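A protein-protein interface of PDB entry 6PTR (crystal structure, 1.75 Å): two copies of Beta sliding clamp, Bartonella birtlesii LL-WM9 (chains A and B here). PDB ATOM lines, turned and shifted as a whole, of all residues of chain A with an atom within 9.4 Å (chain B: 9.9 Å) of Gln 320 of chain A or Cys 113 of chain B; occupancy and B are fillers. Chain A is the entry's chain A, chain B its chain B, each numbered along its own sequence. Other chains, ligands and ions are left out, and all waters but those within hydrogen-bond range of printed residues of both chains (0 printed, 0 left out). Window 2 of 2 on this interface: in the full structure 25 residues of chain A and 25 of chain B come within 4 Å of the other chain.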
ATOM      1  N   VAL A 273      18.650 -31.241 -19.763  1.00  0.00           N
ATOM      2  CA  VAL A 273      19.088 -30.252 -18.791  1.00  0.00           C
ATOM      3  C   VAL A 273      19.390 -28.961 -19.530  1.00  0.00           C
ATOM      4  O   VAL A 273      19.646 -28.958 -20.731  1.00  0.00           O
ATOM      5  CB  VAL A 273      20.322 -30.726 -17.991  1.00  0.00           C
ATOM      6  CG1 VAL A 273      19.962 -31.933 -17.131  1.00  0.00           C
ATOM      7  CG2 VAL A 273      21.483 -31.077 -18.932  1.00  0.00           C
ATOM      8  N   ASP A 277      23.568 -24.313 -17.176  1.00  0.00           N
ATOM      9  CA  ASP A 277      23.387 -24.619 -15.761  1.00  0.00           C
ATOM     10  C   ASP A 277      24.034 -25.947 -15.398  1.00  0.00           C
ATOM     11  O   ASP A 277      24.632 -26.075 -14.324  1.00  0.00           O
ATOM     12  CB  ASP A 277      21.903 -24.660 -15.402  1.00  0.00           C
ATOM     13  CG  ASP A 277      21.236 -23.325 -15.563  1.00  0.00           C
ATOM     14  OD1 ASP A 277      21.964 -22.316 -15.655  1.00  0.00           O
ATOM     15  OD2 ASP A 277      19.986 -23.286 -15.596  1.00  0.00           O
ATOM     16  N   PHE A 278      23.872 -26.958 -16.261  1.00  0.00           N
ATOM     17  CA  PHE A 278      24.491 -28.264 -16.034  1.00  0.00           C
ATOM     18  C   PHE A 278      26.007 -28.156 -16.038  1.00  0.00           C
ATOM     19  O   PHE A 278      26.679 -28.705 -15.156  1.00  0.00           O
ATOM     20  CB  PHE A 278      24.043 -29.248 -17.113  1.00  0.00           C
ATOM     21  CG  PHE A 278      24.673 -30.620 -17.005  1.00  0.00           C
ATOM     22  CD1 PHE A 278      24.227 -31.538 -16.067  1.00  0.00           C
ATOM     23  CD2 PHE A 278      25.671 -30.999 -17.877  1.00  0.00           C
ATOM     24  CE1 PHE A 278      24.819 -32.819 -15.990  1.00  0.00           C
ATOM     25  CE2 PHE A 278      26.261 -32.267 -17.814  1.00  0.00           C
ATOM     26  CZ  PHE A 278      25.810 -33.176 -16.879  1.00  0.00           C
ATOM     27  N   SER A 280      27.884 -25.544 -15.498  1.00  0.00           N
ATOM     28  CA  SER A 280      28.389 -24.789 -14.353  1.00  0.00           C
ATOM     29  C   SER A 280      28.300 -25.615 -13.075  1.00  0.00           C
ATOM     30  O   SER A 280      29.193 -25.554 -12.231  1.00  0.00           O
ATOM     31  CB  SER A 280      27.624 -23.471 -14.201  1.00  0.00           C
ATOM     32  OG  SER A 280      27.800 -22.665 -15.349  1.00  0.00           O
ATOM     33  N   ALA A 281      27.226 -26.398 -12.924  1.00  0.00           N
ATOM     34  CA  ALA A 281      27.082 -27.220 -11.723  1.00  0.00           C
ATOM     35  C   ALA A 281      28.148 -28.308 -11.659  1.00  0.00           C
ATOM     36  O   ALA A 281      28.738 -28.539 -10.596  1.00  0.00           O
ATOM     37  CB  ALA A 281      25.682 -27.837 -11.664  1.00  0.00           C
ATOM     38  N   VAL A 282      28.402 -28.990 -12.783  1.00  0.00           N
ATOM     39  CA  VAL A 282      29.459 -29.997 -12.841  1.00  0.00           C
ATOM     40  C   VAL A 282      30.808 -29.360 -12.539  1.00  0.00           C
ATOM     41  O   VAL A 282      31.624 -29.910 -11.790  1.00  0.00           O
ATOM     42  CB  VAL A 282      29.460 -30.683 -14.226  1.00  0.00           C
ATOM     43  CG1 VAL A 282      30.717 -31.543 -14.415  1.00  0.00           C
ATOM     44  CG2 VAL A 282      28.198 -31.540 -14.404  1.00  0.00           C
ATOM     45  N   ARG A 284      31.373 -26.730 -10.725  1.00  0.00           N
ATOM     46  CA  ARG A 284      31.435 -26.405  -9.303  1.00  0.00           C
ATOM     47  C   ARG A 284      31.711 -27.638  -8.452  1.00  0.00           C
ATOM     48  O   ARG A 284      32.623 -27.628  -7.623  1.00  0.00           O
ATOM     49  CB  ARG A 284      30.146 -25.717  -8.843  1.00  0.00           C
ATOM     50  CG  ARG A 284      30.057 -24.264  -9.305  1.00  0.00           C
ATOM     51  CD  ARG A 284      28.835 -23.499  -8.742  1.00  0.00           C
ATOM     52  NE  ARG A 284      27.567 -24.202  -8.914  1.00  0.00           N
ATOM     53  CZ  ARG A 284      26.726 -23.991  -9.927  1.00  0.00           C
ATOM     54  NH1 ARG A 284      27.021 -23.092 -10.867  1.00  0.00           N
ATOM     55  NH2 ARG A 284      25.580 -24.659  -9.989  1.00  0.00           N
ATOM     56  N   VAL A 285      30.917 -28.697  -8.606  1.00  0.00           N
ATOM     57  CA  VAL A 285      31.123 -29.832  -7.707  1.00  0.00           C
ATOM     58  C   VAL A 285      32.438 -30.543  -7.994  1.00  0.00           C
ATOM     59  O   VAL A 285      33.023 -31.135  -7.081  1.00  0.00           O
ATOM     60  CB  VAL A 285      29.927 -30.812  -7.733  1.00  0.00           C
ATOM     61  CG1 VAL A 285      28.627 -30.081  -7.302  1.00  0.00           C
ATOM     62  CG2 VAL A 285      29.740 -31.471  -9.088  1.00  0.00           C
ATOM     63  N   LYS A 297      28.582 -38.384  -9.544  1.00  0.00           N
ATOM     64  CA  LYS A 297      27.383 -39.214  -9.551  1.00  0.00           C
ATOM     65  C   LYS A 297      26.165 -38.357  -9.870  1.00  0.00           C
ATOM     66  O   LYS A 297      25.938 -37.318  -9.240  1.00  0.00           O
ATOM     67  CB  LYS A 297      27.179 -39.917  -8.206  1.00  0.00           C
ATOM     68  CG  LYS A 297      25.819 -40.599  -8.096  1.00  0.00           C
ATOM     69  CD  LYS A 297      25.761 -41.563  -6.932  1.00  0.00           C
ATOM     70  CE  LYS A 297      25.963 -40.844  -5.641  1.00  0.00           C
ATOM     71  NZ  LYS A 297      25.591 -41.724  -4.494  1.00  0.00           N
ATOM     72  N   THR A 299      22.203 -38.389  -9.800  1.00  0.00           N
ATOM     73  CA  THR A 299      21.018 -39.066  -9.283  1.00  0.00           C
ATOM     74  C   THR A 299      19.822 -38.430  -9.965  1.00  0.00           C
ATOM     75  O   THR A 299      19.503 -37.267  -9.698  1.00  0.00           O
ATOM     76  CB  THR A 299      20.930 -38.956  -7.770  1.00  0.00           C
ATOM     77  OG1 THR A 299      22.098 -39.554  -7.203  1.00  0.00           O
ATOM     78  CG2 THR A 299      19.700 -39.707  -7.268  1.00  0.00           C
ATOM     79  N   GLU A 301      15.940 -38.209 -11.027  1.00  0.00           N
ATOM     80  CA  GLU A 301      14.568 -38.544 -10.672  1.00  0.00           C
ATOM     81  C   GLU A 301      13.644 -37.676 -11.517  1.00  0.00           C
ATOM     82  O   GLU A 301      14.102 -36.833 -12.293  1.00  0.00           O
ATOM     83  CB  GLU A 301      14.301 -38.346  -9.173  1.00  0.00           C
ATOM     84  CG  GLU A 301      15.196 -39.201  -8.293  1.00  0.00           C
ATOM     85  CD  GLU A 301      15.299 -38.670  -6.880  1.00  0.00           C
ATOM     86  OE1 GLU A 301      14.243 -38.378  -6.271  1.00  0.00           O
ATOM     87  OE2 GLU A 301      16.440 -38.530  -6.386  1.00  0.00           O
ATOM     88  N   HIS A 302      12.343 -37.897 -11.384  1.00  0.00           N
ATOM     89  CA  HIS A 302      11.401 -37.120 -12.177  1.00  0.00           C
ATOM     90  C   HIS A 302      11.621 -35.634 -11.960  1.00  0.00           C
ATOM     91  O   HIS A 302      11.546 -35.144 -10.827  1.00  0.00           O
ATOM     92  CB  HIS A 302       9.972 -37.502 -11.823  1.00  0.00           C
ATOM     93  CG  HIS A 302       9.599 -38.864 -12.301  1.00  0.00           C
ATOM     94  ND1 HIS A 302       8.430 -39.490 -11.938  1.00  0.00           N
ATOM     95  CD2 HIS A 302      10.252 -39.726 -13.119  1.00  0.00           C
ATOM     96  CE1 HIS A 302       8.373 -40.678 -12.511  1.00  0.00           C
ATOM     97  NE2 HIS A 302       9.467 -40.847 -13.229  1.00  0.00           N
ATOM     98  N   GLY A 303      11.918 -34.934 -13.049  1.00  0.00           N
ATOM     99  CA  GLY A 303      12.031 -33.495 -13.037  1.00  0.00           C
ATOM    100  C   GLY A 303      13.242 -32.929 -12.334  1.00  0.00           C
ATOM    101  O   GLY A 303      13.276 -31.716 -12.097  1.00  0.00           O
ATOM    102  N   GLN A 304      14.254 -33.742 -12.031  1.00  0.00           N
ATOM    103  CA  GLN A 304      15.271 -33.336 -11.067  1.00  0.00           C
ATOM    104  C   GLN A 304      16.573 -34.101 -11.282  1.00  0.00           C
ATOM    105  O   GLN A 304      16.564 -35.310 -11.516  1.00  0.00           O
ATOM    106  CB  GLN A 304      14.725 -33.563  -9.649  1.00  0.00           C
ATOM    107  CG  GLN A 304      15.708 -33.480  -8.536  1.00  0.00           C
ATOM    108  CD  GLN A 304      15.040 -33.741  -7.205  1.00  0.00           C
ATOM    109  OE1 GLN A 304      15.563 -34.473  -6.370  1.00  0.00           O
ATOM    110  NE2 GLN A 304      13.866 -33.151  -7.008  1.00  0.00           N
ATOM    111  N   LEU A 305      17.695 -33.393 -11.188  1.00  0.00           N
ATOM    112  CA  LEU A 305      19.009 -34.013 -11.253  1.00  0.00           C
ATOM    113  C   LEU A 305      19.830 -33.545 -10.057  1.00  0.00           C
ATOM    114  O   LEU A 305      19.988 -32.336  -9.857  1.00  0.00           O
ATOM    115  CB  LEU A 305      19.718 -33.628 -12.556  1.00  0.00           C
ATOM    116  CG  LEU A 305      21.164 -34.071 -12.676  1.00  0.00           C
ATOM    117  CD1 LEU A 305      21.177 -35.597 -12.765  1.00  0.00           C
ATOM    118  CD2 LEU A 305      21.822 -33.460 -13.905  1.00  0.00           C
ATOM    119  N   LYS A 306      20.352 -34.492  -9.277  1.00  0.00           N
ATOM    120  CA  LYS A 306      21.298 -34.200  -8.209  1.00  0.00           C
ATOM    121  C   LYS A 306      22.682 -34.660  -8.633  1.00  0.00           C
ATOM    122  O   LYS A 306      22.825 -35.709  -9.269  1.00  0.00           O
ATOM    123  CB  LYS A 306      20.890 -34.888  -6.886  1.00  0.00           C
ATOM    124  CG  LYS A 306      19.698 -34.277  -6.205  1.00  0.00           C
ATOM    125  CD  LYS A 306      19.339 -35.078  -4.942  1.00  0.00           C
ATOM    126  CE  LYS A 306      18.072 -34.579  -4.277  1.00  0.00           C
ATOM    127  NZ  LYS A 306      17.727 -35.413  -3.089  1.00  0.00           N
ATOM    128  N   LEU A 307      23.698 -33.858  -8.312  1.00  0.00           N
ATOM    129  CA  LEU A 307      25.086 -34.181  -8.623  1.00  0.00           C
ATOM    130  C   LEU A 307      25.854 -34.307  -7.317  1.00  0.00           C
ATOM    131  O   LEU A 307      25.642 -33.514  -6.399  1.00  0.00           O
ATOM    132  CB  LEU A 307      25.738 -33.095  -9.483  1.00  0.00           C
ATOM    133  CG  LEU A 307      25.059 -32.658 -10.772  1.00  0.00           C
ATOM    134  CD1 LEU A 307      25.876 -31.562 -11.452  1.00  0.00           C
ATOM    135  CD2 LEU A 307      24.985 -33.846 -11.687  1.00  0.00           C
ATOM    136  N   VAL A 308      26.725 -35.316  -7.213  1.00  0.00           N
ATOM    137  CA  VAL A 308      27.546 -35.483  -6.014  1.00  0.00           C
ATOM    138  C   VAL A 308      28.948 -35.899  -6.425  1.00  0.00           C
ATOM    139  O   VAL A 308      29.120 -36.781  -7.274  1.00  0.00           O
ATOM    140  CB  VAL A 308      26.962 -36.510  -5.019  1.00  0.00           C
ATOM    141  CG1 VAL A 308      27.820 -36.562  -3.755  1.00  0.00           C
ATOM    142  CG2 VAL A 308      25.566 -36.131  -4.613  1.00  0.00           C
ATOM    143  N   ALA A 317      30.847 -32.526  -2.381  1.00  0.00           N
ATOM    144  CA  ALA A 317      30.243 -31.412  -3.098  1.00  0.00           C
ATOM    145  C   ALA A 317      28.962 -31.916  -3.741  1.00  0.00           C
ATOM    146  O   ALA A 317      28.964 -32.974  -4.366  1.00  0.00           O
ATOM    147  CB  ALA A 317      31.196 -30.876  -4.171  1.00  0.00           C
ATOM    148  N   GLU A 318      27.881 -31.172  -3.592  1.00  0.00           N
ATOM    149  CA  GLU A 318      26.597 -31.562  -4.158  1.00  0.00           C
ATOM    150  C   GLU A 318      25.952 -30.357  -4.816  1.00  0.00           C
ATOM    151  O   GLU A 318      26.161 -29.214  -4.399  1.00  0.00           O
ATOM    152  CB  GLU A 318      25.628 -32.096  -3.091  1.00  0.00           C
ATOM    153  CG  GLU A 318      26.116 -33.308  -2.336  1.00  0.00           C
ATOM    154  CD  GLU A 318      25.160 -33.719  -1.224  1.00  0.00           C
ATOM    155  OE1 GLU A 318      24.001 -33.245  -1.219  1.00  0.00           O
ATOM    156  OE2 GLU A 318      25.575 -34.514  -0.354  1.00  0.00           O
ATOM    157  N   ASP A 319      25.126 -30.625  -5.822  1.00  0.00           N
ATOM    158  CA  ASP A 319      24.331 -29.577  -6.444  1.00  0.00           C
ATOM    159  C   ASP A 319      23.047 -30.218  -6.947  1.00  0.00           C
ATOM    160  O   ASP A 319      22.904 -31.441  -6.950  1.00  0.00           O
ATOM    161  CB  ASP A 319      25.098 -28.893  -7.580  1.00  0.00           C
ATOM    162  CG  ASP A 319      24.729 -27.431  -7.750  1.00  0.00           C
ATOM    163  OD1 ASP A 319      23.559 -27.051  -7.526  1.00  0.00           O
ATOM    164  OD2 ASP A 319      25.630 -26.653  -8.122  1.00  0.00           O
ATOM    165  N   GLN A 320      22.091 -29.380  -7.317  1.00  0.00           N
ATOM    166  CA  GLN A 320      20.807 -29.886  -7.784  1.00  0.00           C
ATOM    167  C   GLN A 320      20.293 -28.985  -8.895  1.00  0.00           C
ATOM    168  O   GLN A 320      20.400 -27.758  -8.810  1.00  0.00           O
ATOM    169  CB  GLN A 320      19.811 -29.970  -6.631  1.00  0.00           C
ATOM    170  CG  GLN A 320      18.447 -30.491  -7.043  1.00  0.00           C
ATOM    171  CD  GLN A 320      17.516 -30.639  -5.859  1.00  0.00           C
ATOM    172  OE1 GLN A 320      17.922 -31.085  -4.783  1.00  0.00           O
ATOM    173  NE2 GLN A 320      16.268 -30.246  -6.047  1.00  0.00           N
ATOM    174  N   LEU A 321      19.760 -29.601  -9.950  1.00  0.00           N
ATOM    175  CA  LEU A 321      19.285 -28.886 -11.121  1.00  0.00           C
ATOM    176  C   LEU A 321      17.869 -29.314 -11.443  1.00  0.00           C
ATOM    177  O   LEU A 321      17.502 -30.469 -11.235  1.00  0.00           O
ATOM    178  CB  LEU A 321      20.144 -29.196 -12.349  1.00  0.00           C
ATOM    179  CG  LEU A 321      21.588 -28.760 -12.241  1.00  0.00           C
ATOM    180  CD1 LEU A 321      22.371 -29.323 -13.411  1.00  0.00           C
ATOM    181  CD2 LEU A 321      21.619 -27.234 -12.207  1.00  0.00           C
ATOM    182  N   ALA A 322      17.091 -28.389 -11.994  1.00  0.00           N
ATOM    183  CA  ALA A 322      15.876 -28.809 -12.673  1.00  0.00           C
ATOM    184  C   ALA A 322      16.239 -29.576 -13.944  1.00  0.00           C
ATOM    185  O   ALA A 322      17.281 -29.353 -14.574  1.00  0.00           O
ATOM    186  CB  ALA A 322      14.992 -27.611 -13.009  1.00  0.00           C
ATOM    187  N   ALA A 323      15.380 -30.519 -14.307  1.00  0.00           N
ATOM    188  CA  ALA A 323      15.629 -31.324 -15.489  1.00  0.00           C
ATOM    189  C   ALA A 323      14.289 -31.765 -16.035  1.00  0.00           C
ATOM    190  O   ALA A 323      13.272 -31.716 -15.338  1.00  0.00           O
ATOM    191  CB  ALA A 323      16.502 -32.542 -15.191  1.00  0.00           C
ATOM    192  N   LEU B  89      31.688 -19.551  -7.715  1.00  0.00           N
ATOM    193  CA  LEU B  89      30.344 -19.183  -7.295  1.00  0.00           C
ATOM    194  C   LEU B  89      29.975 -17.817  -7.867  1.00  0.00           C
ATOM    195  O   LEU B  89      30.848 -16.963  -8.070  1.00  0.00           O
ATOM    196  CB  LEU B  89      30.245 -19.166  -5.773  1.00  0.00           C
ATOM    197  CG  LEU B  89      30.536 -20.520  -5.129  1.00  0.00           C
ATOM    198  CD1 LEU B  89      30.636 -20.393  -3.603  1.00  0.00           C
ATOM    199  CD2 LEU B  89      29.458 -21.531  -5.522  1.00  0.00           C
ATOM    200  N   PRO B  90      28.690 -17.594  -8.147  1.00  0.00           N
ATOM    201  CA  PRO B  90      28.305 -16.438  -8.966  1.00  0.00           C
ATOM    202  C   PRO B  90      28.431 -15.102  -8.241  1.00  0.00           C
ATOM    203  O   PRO B  90      28.054 -14.954  -7.077  1.00  0.00           O
ATOM    204  CB  PRO B  90      26.845 -16.737  -9.335  1.00  0.00           C
ATOM    205  CG  PRO B  90      26.377 -17.716  -8.325  1.00  0.00           C
ATOM    206  CD  PRO B  90      27.572 -18.537  -7.956  1.00  0.00           C
ATOM    207  N   SER B  93      25.946 -13.372  -5.545  1.00  0.00           N
ATOM    208  CA  SER B  93      25.313 -14.379  -4.711  1.00  0.00           C
ATOM    209  C   SER B  93      25.792 -14.236  -3.268  1.00  0.00           C
ATOM    210  O   SER B  93      26.710 -13.466  -2.966  1.00  0.00           O
ATOM    211  CB  SER B  93      25.634 -15.774  -5.233  1.00  0.00           C
ATOM    212  OG  SER B  93      27.036 -15.991  -5.208  1.00  0.00           O
ATOM    213  N   GLU B  94      25.152 -14.989  -2.370  1.00  0.00           N
ATOM    214  CA  GLU B  94      25.566 -15.084  -0.976  1.00  0.00           C
ATOM    215  C   GLU B  94      26.068 -16.489  -0.684  1.00  0.00           C
ATOM    216  O   GLU B  94      25.688 -17.457  -1.342  1.00  0.00           O
ATOM    217  CB  GLU B  94      24.417 -14.748  -0.017  1.00  0.00           C
ATOM    218  CG  GLU B  94      24.056 -13.282   0.005  1.00  0.00           C
ATOM    219  CD  GLU B  94      22.997 -12.958   1.038  1.00  0.00           C
ATOM    220  OE1 GLU B  94      22.087 -13.795   1.251  1.00  0.00           O
ATOM    221  OE2 GLU B  94      23.082 -11.861   1.635  1.00  0.00           O
ATOM    222  N   ILE B  95      26.925 -16.591   0.321  1.00  0.00           N
ATOM    223  CA  ILE B  95      27.527 -17.860   0.714  1.00  0.00           C
ATOM    224  C   ILE B  95      27.319 -18.022   2.206  1.00  0.00           C
ATOM    225  O   ILE B  95      27.656 -17.118   2.971  1.00  0.00           O
ATOM    226  CB  ILE B  95      29.032 -17.903   0.410  1.00  0.00           C
ATOM    227  CG1 ILE B  95      29.303 -17.589  -1.055  1.00  0.00           C
ATOM    228  CG2 ILE B  95      29.588 -19.265   0.756  1.00  0.00           C
ATOM    229  CD1 ILE B  95      30.784 -17.390  -1.312  1.00  0.00           C
ATOM    230  N   SER B 108      30.677 -26.467   6.223  1.00  0.00           N
ATOM    231  CA  SER B 108      29.719 -26.455   5.131  1.00  0.00           C
ATOM    232  C   SER B 108      29.794 -25.129   4.392  1.00  0.00           C
ATOM    233  O   SER B 108      29.927 -24.060   5.003  1.00  0.00           O
ATOM    234  CB  SER B 108      28.308 -26.690   5.682  1.00  0.00           C
ATOM    235  OG  SER B 108      27.309 -26.371   4.738  1.00  0.00           O
ATOM    236  N   ILE B 109      29.713 -25.200   3.064  1.00  0.00           N
ATOM    237  CA  ILE B 109      29.624 -24.024   2.214  1.00  0.00           C
ATOM    238  C   ILE B 109      28.374 -24.195   1.379  1.00  0.00           C
ATOM    239  O   ILE B 109      28.271 -25.168   0.624  1.00  0.00           O
ATOM    240  CB  ILE B 109      30.848 -23.870   1.310  1.00  0.00           C
ATOM    241  CG1 ILE B 109      32.155 -23.856   2.111  1.00  0.00           C
ATOM    242  CG2 ILE B 109      30.710 -22.621   0.468  1.00  0.00           C
ATOM    243  CD1 ILE B 109      33.351 -24.009   1.231  1.00  0.00           C
ATOM    244  N   VAL B 110      27.418 -23.275   1.512  1.00  0.00           N
ATOM    245  CA  VAL B 110      26.177 -23.359   0.750  1.00  0.00           C
ATOM    246  C   VAL B 110      26.012 -22.091  -0.075  1.00  0.00           C
ATOM    247  O   VAL B 110      26.078 -20.977   0.456  1.00  0.00           O
ATOM    248  CB  VAL B 110      24.955 -23.574   1.663  1.00  0.00           C
ATOM    249  CG1 VAL B 110      23.679 -23.499   0.856  1.00  0.00           C
ATOM    250  CG2 VAL B 110      25.055 -24.930   2.362  1.00  0.00           C
ATOM    251  N   SER B 111      25.781 -22.258  -1.371  1.00  0.00           N
ATOM    252  CA  SER B 111      25.490 -21.134  -2.249  1.00  0.00           C
ATOM    253  C   SER B 111      24.417 -21.615  -3.214  1.00  0.00           C
ATOM    254  O   SER B 111      24.699 -22.437  -4.092  1.00  0.00           O
ATOM    255  CB  SER B 111      26.741 -20.668  -2.993  1.00  0.00           C
ATOM    256  OG  SER B 111      26.394 -19.857  -4.106  1.00  0.00           O
ATOM    257  N   GLY B 112      23.191 -21.139  -3.022  1.00  0.00           N
ATOM    258  CA  GLY B 112      22.096 -21.616  -3.852  1.00  0.00           C
ATOM    259  C   GLY B 112      21.852 -23.070  -3.529  1.00  0.00           C
ATOM    260  O   GLY B 112      21.779 -23.465  -2.359  1.00  0.00           O
ATOM    261  N   CYS B 113      21.770 -23.892  -4.573  1.00  0.00           N
ATOM    262  CA  CYS B 113      21.690 -25.332  -4.396  1.00  0.00           C
ATOM    263  C   CYS B 113      23.054 -25.991  -4.275  1.00  0.00           C
ATOM    264  O   CYS B 113      23.117 -27.206  -4.069  1.00  0.00           O
ATOM    265  CB  CYS B 113      20.927 -25.959  -5.557  1.00  0.00           C
ATOM    266  SG  CYS B 113      19.226 -25.479  -5.532  1.00  0.00           S
ATOM    267  N   THR B 114      24.143 -25.234  -4.385  1.00  0.00           N
ATOM    268  CA  THR B 114      25.469 -25.836  -4.312  1.00  0.00           C
ATOM    269  C   THR B 114      25.879 -25.987  -2.851  1.00  0.00           C
ATOM    270  O   THR B 114      25.776 -25.034  -2.075  1.00  0.00           O
ATOM    271  CB  THR B 114      26.501 -24.976  -5.042  1.00  0.00           C
ATOM    272  OG1 THR B 114      25.993 -24.571  -6.311  1.00  0.00           O
ATOM    273  CG2 THR B 114      27.761 -25.773  -5.258  1.00  0.00           C
ATOM    274  N   HIS B 115      26.354 -27.174  -2.474  1.00  0.00           N
ATOM    275  CA  HIS B 115      26.703 -27.425  -1.074  1.00  0.00           C
ATOM    276  C   HIS B 115      27.987 -28.229  -1.003  1.00  0.00           C
ATOM    277  O   HIS B 115      28.041 -29.363  -1.494  1.00  0.00           O
ATOM    278  CB  HIS B 115      25.558 -28.159  -0.361  1.00  0.00           C
ATOM    279  CG  HIS B 115      25.923 -28.680   0.998  1.00  0.00           C
ATOM    280  ND1 HIS B 115      25.484 -29.901   1.469  1.00  0.00           N
ATOM    281  CD2 HIS B 115      26.675 -28.146   1.991  1.00  0.00           C
ATOM    282  CE1 HIS B 115      25.958 -30.100   2.685  1.00  0.00           C
ATOM    283  NE2 HIS B 115      26.680 -29.049   3.027  1.00  0.00           N
ATOM    284  N   PHE B 116      29.015 -27.647  -0.377  1.00  0.00           N
ATOM    285  CA  PHE B 116      30.283 -28.326  -0.120  1.00  0.00           C
ATOM    286  C   PHE B 116      30.383 -28.664   1.363  1.00  0.00           C
ATOM    287  O   PHE B 116      29.908 -27.908   2.210  1.00  0.00           O
ATOM    288  CB  PHE B 116      31.485 -27.443  -0.499  1.00  0.00           C
ATOM    289  CG  PHE B 116      31.549 -27.078  -1.961  1.00  0.00           C
ATOM    290  CD1 PHE B 116      30.883 -25.959  -2.441  1.00  0.00           C
ATOM    291  CD2 PHE B 116      32.288 -27.853  -2.845  1.00  0.00           C
ATOM    292  CE1 PHE B 116      30.928 -25.625  -3.807  1.00  0.00           C
ATOM    293  CE2 PHE B 116      32.337 -27.532  -4.199  1.00  0.00           C
ATOM    294  CZ  PHE B 116      31.670 -26.407  -4.674  1.00  0.00           C
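OG1 of Thr 114 of chain B is in hydrogen-bond range of NE of Arg 284 of chain A (3.1 Å). O of His 115 of chain B sits at hydrogen-bond distance from N of Glu 318 of chain A, at 2.8 Å. The side-chain hydroxyl of Thr 114 of chain B is in hydrogen-bond range of the side-chain carboxylate of Asp 319 of chain A (2.8 Å). The side-chain carboxylate (OD1) of Asp 319 of chain A lies close to the backbone carbonyl oxygen (O) of Cys 113 of chain B (3.5 Å).
NH2 of Arg 284 of chain A is in salt-bridge range of OD2 of Asp 319 of chain A, 2.7 Å away. The backbone NH (N) of Leu 307 of chain A is in hydrogen-bond range of the backbone carbonyl oxygen (O) of Asp 319 of chain A (2.9 Å). OG of Ser 108 of chain B sits at hydrogen-bond distance from NE2 of His 115 of chain B (3.2 Å). The backbone NH of Phe 116 of chain B sits at hydrogen-bond distance from the backbone carbonyl oxygen of Ile 109 of chain B (2.8 Å). The side-chain hydroxyl (OG1) of Thr 114 of chain B lies close to the backbone carbonyl oxygen (O) of Ser 111 of chain B (3.3 Å).
Among the printed residues, pairs that only touch across the chains: Arg 284 of chain A with Leu 89 of chain B (3.8 Å), Arg 284 of chain A with Phe 116 of chain B (3.3 Å), Ala 317 of chain A with His 115 of chain B (3.4 Å), Ala 317 of chain A with Phe 116 of chain B (3.5 Å), Glu 318 of chain A with Cys 113 of chain B (3.7 Å), Glu 318 of chain A with Thr 114 of chain B (3.4 Å) and Gln 320 of chain A with Cys 113 of chain B (3.8 Å).
Of chain B, only Cys 113 (3.8 Å) comes within 4 Å of Gln 320 of chain A. Cys 113 of chain B touches just these residues of chain A: Glu 318 (3.7 Å), Asp 319 (3.5 Å) and Gln 320 (3.8 Å). Asp 319 of chain A touches two residues of chain B. No residue of chain B comes within 4 Å of Leu 321 of chain A. No residue of chain A comes within 4 Å of Gly 112 of chain B. Of chain A, only Arg 284, Glu 318 and Asp 319 come within 4 Å of Thr 114 of chain B. Printed residues of chain B within 4 Å of Glu 318 of chain A: Cys 113 (3.7 Å), Thr 114 (3.4 Å) and His 115 (2.8 Å). Printed residues of chain B within 4 Å of Ala 317 of chain A: His 115 (3.4 Å) and Phe 116 (3.5 Å). Printed residues of chain B within 4 Å of Arg 284 of chain A: Leu 89, Thr 114 and Phe 116. Printed residues of chain A within 4 Å of Phe 116 of chain B: Arg 284 and Ala 317. Of the printed residues of chain A, Leu 89 of chain B touches Arg 284 (3.8 Å). Glu 94 of chain B touches none of the printed residues of chain A. The nearest residue of chain A that does not touch Cys 113 of chain B is Leu 321 of chain A (5.8 Å). The nearest printed residue of chain B that does not touch Arg 284 of chain A is Pro 90 of chain B (5.2 Å).
Of the 14 printed residues of chain B, 5 touch a printed residue of chain A.
No position is printed for both chains. Of the 11 pairs that touch across the chains among the printed residues, none has its exchanged pair printed and touching as well.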
